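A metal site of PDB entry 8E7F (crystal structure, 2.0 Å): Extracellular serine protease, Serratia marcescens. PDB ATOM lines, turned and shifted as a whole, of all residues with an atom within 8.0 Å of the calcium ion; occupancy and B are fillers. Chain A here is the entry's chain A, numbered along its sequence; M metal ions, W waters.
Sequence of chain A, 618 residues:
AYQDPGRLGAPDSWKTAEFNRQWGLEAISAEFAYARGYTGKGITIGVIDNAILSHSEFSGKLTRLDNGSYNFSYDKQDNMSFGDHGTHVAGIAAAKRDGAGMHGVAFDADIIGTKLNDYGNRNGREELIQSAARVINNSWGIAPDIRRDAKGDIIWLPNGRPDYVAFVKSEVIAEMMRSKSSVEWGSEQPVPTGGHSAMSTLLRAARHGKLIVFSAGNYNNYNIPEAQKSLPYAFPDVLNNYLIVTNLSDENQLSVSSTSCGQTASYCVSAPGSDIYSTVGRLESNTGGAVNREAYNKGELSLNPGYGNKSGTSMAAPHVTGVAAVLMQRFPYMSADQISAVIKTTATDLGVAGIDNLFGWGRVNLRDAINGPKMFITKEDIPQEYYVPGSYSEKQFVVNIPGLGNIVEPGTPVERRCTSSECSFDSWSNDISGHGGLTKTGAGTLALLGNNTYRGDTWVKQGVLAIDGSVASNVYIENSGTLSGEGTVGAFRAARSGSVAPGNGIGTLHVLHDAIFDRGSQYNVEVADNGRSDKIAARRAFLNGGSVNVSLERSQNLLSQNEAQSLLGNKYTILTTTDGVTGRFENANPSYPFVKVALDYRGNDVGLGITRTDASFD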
ATOM      1  N   THR A 348       3.239   3.667 -10.766  1.00  0.00           N
ATOM      2  CA  THR A 348       3.154   3.899  -9.308  1.00  0.00           C
ATOM      3  C   THR A 348       2.083   2.951  -8.743  1.00  0.00           C
ATOM      4  O   THR A 348       0.931   3.087  -9.125  1.00  0.00           O
ATOM      5  CB  THR A 348       2.892   5.370  -9.006  1.00  0.00           C
ATOM      6  OG1 THR A 348       3.992   6.117  -9.518  1.00  0.00           O
ATOM      7  CG2 THR A 348       2.748   5.666  -7.520  1.00  0.00           C
ATOM      8  N   ASP A 349       2.466   2.042  -7.851  1.00  0.00           N
ATOM      9  CA  ASP A 349       1.522   1.078  -7.208  1.00  0.00           C
ATOM     10  C   ASP A 349       0.412   1.857  -6.479  1.00  0.00           C
ATOM     11  O   ASP A 349       0.717   2.823  -5.815  1.00  0.00           O
ATOM     12  CB  ASP A 349       2.267   0.152  -6.253  1.00  0.00           C
ATOM     13  CG  ASP A 349       1.476  -1.054  -5.808  1.00  0.00           C
ATOM     14  OD1 ASP A 349       2.113  -1.980  -5.225  1.00  0.00           O
ATOM     15  OD2 ASP A 349       0.228  -1.101  -6.066  1.00  0.00           O
ATOM     16  N   LEU A 350      -0.848   1.535  -6.750  1.00  0.00           N
ATOM     17  CA  LEU A 350      -2.015   2.166  -6.097  1.00  0.00           C
ATOM     18  C   LEU A 350      -2.815   1.058  -5.406  1.00  0.00           C
ATOM     19  O   LEU A 350      -2.675  -0.111  -5.777  1.00  0.00           O
ATOM     20  CB  LEU A 350      -2.902   2.899  -7.109  1.00  0.00           C
ATOM     21  CG  LEU A 350      -2.286   4.065  -7.880  1.00  0.00           C
ATOM     22  CD1 LEU A 350      -3.314   4.709  -8.796  1.00  0.00           C
ATOM     23  CD2 LEU A 350      -1.708   5.102  -6.935  1.00  0.00           C
ATOM     24  N   GLY A 351      -3.623   1.451  -4.438  1.00  0.00           N
ATOM     25  CA  GLY A 351      -4.559   0.571  -3.715  1.00  0.00           C
ATOM     26  C   GLY A 351      -3.815  -0.542  -3.035  1.00  0.00           C
ATOM     27  O   GLY A 351      -2.754  -0.289  -2.483  1.00  0.00           O
ATOM     28  N   VAL A 352      -4.340  -1.744  -3.108  1.00  0.00           N
ATOM     29  CA  VAL A 352      -3.713  -2.955  -2.503  1.00  0.00           C
ATOM     30  C   VAL A 352      -2.334  -3.155  -3.135  1.00  0.00           C
ATOM     31  O   VAL A 352      -2.225  -3.122  -4.388  1.00  0.00           O
ATOM     32  CB  VAL A 352      -4.659  -4.153  -2.711  1.00  0.00           C
ATOM     33  CG1 VAL A 352      -3.997  -5.484  -2.439  1.00  0.00           C
ATOM     34  CG2 VAL A 352      -5.929  -3.971  -1.899  1.00  0.00           C
ATOM     35  N   ALA A 353      -1.313  -3.412  -2.315  1.00  0.00           N
ATOM     36  CA  ALA A 353       0.093  -3.589  -2.750  1.00  0.00           C
ATOM     37  C   ALA A 353       0.165  -4.589  -3.906  1.00  0.00           C
ATOM     38  O   ALA A 353      -0.555  -5.581  -3.930  1.00  0.00           O
ATOM     39  CB  ALA A 353       0.939  -4.042  -1.596  1.00  0.00           C
ATOM     40  N   GLY A 354       1.027  -4.300  -4.877  1.00  0.00           N
ATOM     41  CA  GLY A 354       1.219  -5.163  -6.057  1.00  0.00           C
ATOM     42  C   GLY A 354       0.082  -5.027  -7.057  1.00  0.00           C
ATOM     43  O   GLY A 354      -0.769  -4.121  -6.911  1.00  0.00           O
ATOM     44  N   ILE A 355       0.070  -5.926  -8.035  1.00  0.00           N
ATOM     45  CA  ILE A 355      -0.986  -5.972  -9.082  1.00  0.00           C
ATOM     46  C   ILE A 355      -2.319  -6.279  -8.424  1.00  0.00           C
ATOM     47  O   ILE A 355      -2.397  -7.258  -7.659  1.00  0.00           O
ATOM     48  CB  ILE A 355      -0.611  -6.993 -10.168  1.00  0.00           C
ATOM     49  CG1 ILE A 355       0.670  -6.577 -10.911  1.00  0.00           C
ATOM     50  CG2 ILE A 355      -1.767  -7.216 -11.112  1.00  0.00           C
ATOM     51  CD1 ILE A 355       1.332  -7.719 -11.625  1.00  0.00           C
ATOM     52  N   ASP A 356      -3.347  -5.479  -8.701  1.00  0.00           N
ATOM     53  CA  ASP A 356      -4.690  -5.613  -8.065  1.00  0.00           C
ATOM     54  C   ASP A 356      -5.781  -5.376  -9.124  1.00  0.00           C
ATOM     55  O   ASP A 356      -5.527  -4.719 -10.192  1.00  0.00           O
ATOM     56  CB  ASP A 356      -4.826  -4.669  -6.867  1.00  0.00           C
ATOM     57  CG  ASP A 356      -4.841  -3.201  -7.259  1.00  0.00           C
ATOM     58  OD1 ASP A 356      -3.757  -2.591  -7.309  1.00  0.00           O
ATOM     59  OD2 ASP A 356      -5.906  -2.690  -7.520  1.00  0.00           O
ATOM     60  N   ASN A 357      -6.954  -5.861  -8.800  1.00  0.00           N
ATOM     61  CA  ASN A 357      -8.159  -5.890  -9.682  1.00  0.00           C
ATOM     62  C   ASN A 357      -8.675  -4.476  -9.991  1.00  0.00           C
ATOM     63  O   ASN A 357      -9.440  -4.350 -10.946  1.00  0.00           O
ATOM     64  CB  ASN A 357      -9.241  -6.740  -9.020  1.00  0.00           C
ATOM     65  CG  ASN A 357      -9.685  -6.138  -7.708  1.00  0.00           C
ATOM     66  OD1 ASN A 357      -8.917  -6.065  -6.743  1.00  0.00           O
ATOM     67  ND2 ASN A 357     -10.897  -5.624  -7.681  1.00  0.00           N
ATOM     68  N   LEU A 358      -8.333  -3.449  -9.221  1.00  0.00           N
ATOM     69  CA  LEU A 358      -8.814  -2.072  -9.485  1.00  0.00           C
ATOM     70  C   LEU A 358      -7.847  -1.362 -10.444  1.00  0.00           C
ATOM     71  O   LEU A 358      -8.299  -0.845 -11.460  1.00  0.00           O
ATOM     72  CB  LEU A 358      -8.965  -1.289  -8.183  1.00  0.00           C
ATOM     73  CG  LEU A 358     -10.056  -1.756  -7.201  1.00  0.00           C
ATOM     74  CD1 LEU A 358     -10.254  -0.739  -6.085  1.00  0.00           C
ATOM     75  CD2 LEU A 358     -11.378  -2.018  -7.909  1.00  0.00           C
ATOM     76  N   PHE A 359      -6.560  -1.289 -10.098  1.00  0.00           N
ATOM     77  CA  PHE A 359      -5.592  -0.369 -10.753  1.00  0.00           C
ATOM     78  C   PHE A 359      -4.573  -1.134 -11.601  1.00  0.00           C
ATOM     79  O   PHE A 359      -3.775  -0.484 -12.287  1.00  0.00           O
ATOM     80  CB  PHE A 359      -4.839   0.437  -9.693  1.00  0.00           C
ATOM     81  CG  PHE A 359      -5.711   1.258  -8.785  1.00  0.00           C
ATOM     82  CD1 PHE A 359      -6.241   2.466  -9.198  1.00  0.00           C
ATOM     83  CD2 PHE A 359      -5.931   0.845  -7.472  1.00  0.00           C
ATOM     84  CE1 PHE A 359      -6.983   3.250  -8.331  1.00  0.00           C
ATOM     85  CE2 PHE A 359      -6.681   1.627  -6.599  1.00  0.00           C
ATOM     86  CZ  PHE A 359      -7.212   2.821  -7.039  1.00  0.00           C
ATOM     87  N   GLY A 360      -4.589  -2.465 -11.521  1.00  0.00           N
ATOM     88  CA  GLY A 360      -3.624  -3.324 -12.227  1.00  0.00           C
ATOM     89  C   GLY A 360      -2.218  -3.068 -11.696  1.00  0.00           C
ATOM     90  O   GLY A 360      -2.019  -3.150 -10.456  1.00  0.00           O
ATOM     91  N   TRP A 361      -1.295  -2.704 -12.590  1.00  0.00           N
ATOM     92  CA  TRP A 361       0.082  -2.297 -12.233  1.00  0.00           C
ATOM     93  C   TRP A 361       0.129  -0.897 -11.608  1.00  0.00           C
ATOM     94  O   TRP A 361       1.164  -0.608 -10.980  1.00  0.00           O
ATOM     95  CB  TRP A 361       0.972  -2.351 -13.472  1.00  0.00           C
ATOM     96  CG  TRP A 361       1.247  -3.747 -13.950  1.00  0.00           C
ATOM     97  CD1 TRP A 361       0.468  -4.495 -14.793  1.00  0.00           C
ATOM     98  CD2 TRP A 361       2.398  -4.532 -13.637  1.00  0.00           C
ATOM     99  NE1 TRP A 361       1.062  -5.706 -15.022  1.00  0.00           N
ATOM    100  CE2 TRP A 361       2.254  -5.752 -14.331  1.00  0.00           C
ATOM    101  CE3 TRP A 361       3.552  -4.317 -12.884  1.00  0.00           C
ATOM    102  CZ2 TRP A 361       3.217  -6.768 -14.272  1.00  0.00           C
ATOM    103  CZ3 TRP A 361       4.500  -5.312 -12.798  1.00  0.00           C
ATOM    104  CH2 TRP A 361       4.335  -6.525 -13.499  1.00  0.00           C
ATOM    105  N   GLY A 362      -0.909  -0.082 -11.761  1.00  0.00           N
ATOM    106  CA  GLY A 362      -0.996   1.233 -11.121  1.00  0.00           C
ATOM    107  C   GLY A 362      -0.919   2.384 -12.116  1.00  0.00           C
ATOM    108  O   GLY A 362      -1.202   2.185 -13.290  1.00  0.00           O
ATOM    109  N   ARG A 363      -0.568   3.581 -11.634  1.00  0.00           N
ATOM    110  CA  ARG A 363      -0.651   4.819 -12.421  1.00  0.00           C
ATOM    111  C   ARG A 363       0.610   4.934 -13.275  1.00  0.00           C
ATOM    112  O   ARG A 363       1.724   4.915 -12.697  1.00  0.00           O
ATOM    113  CB  ARG A 363      -0.773   6.050 -11.512  1.00  0.00           C
ATOM    114  CG  ARG A 363      -1.014   7.357 -12.245  1.00  0.00           C
ATOM    115  CD  ARG A 363      -1.071   8.535 -11.292  1.00  0.00           C
ATOM    116  NE  ARG A 363       0.252   8.775 -10.726  1.00  0.00           N
ATOM    117  CZ  ARG A 363       0.616   8.555  -9.478  1.00  0.00           C
ATOM    118  NH1 ARG A 363      -0.234   8.061  -8.593  1.00  0.00           N
ATOM    119  NH2 ARG A 363       1.861   8.812  -9.103  1.00  0.00           N
HETATM  120 CA    CA M   1      -1.756  -2.078  -6.427  1.00  0.00          CA
HETATM  121  O   HOH W   1      -1.140  -1.301  -8.612  1.00  0.00           O
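Water W1 lies within hydrogen-bond range of O of Gly 360 (2.8 Å), O of Trp 361 (3.4 Å), N of Gly 362 (3.4 Å) and N of Leu 350 (3.4 Å).
Five residues have an atom within 4 Å of the calcium ion: Asp 349, Leu 350, Val 352, Gly 354 and Asp 356.
The side-chain carboxylate (OD2) of Asp 356 lies within hydrogen-bond range of the backbone NH (N) of Phe 359 (3.0 Å).
The side-chain carboxylate (OD2) of Asp 356 lies within hydrogen-bond range of the backbone NH (N) of Leu 358 (3.1 Å).
The side-chain carboxylate (OD2) of Asp 349 is bound to the calcium ion.
OD1 of Asp 356 is bound to the calcium ion (2.2 Å).
O of Leu 350 is bound to the calcium ion.
The calcium ion is bound by O of Gly 354 (2.3 Å).
O of Val 352 is bound to the calcium ion.
Water W1 binds the calcium ion.
The calcium ion has six donor atoms within binding distance.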
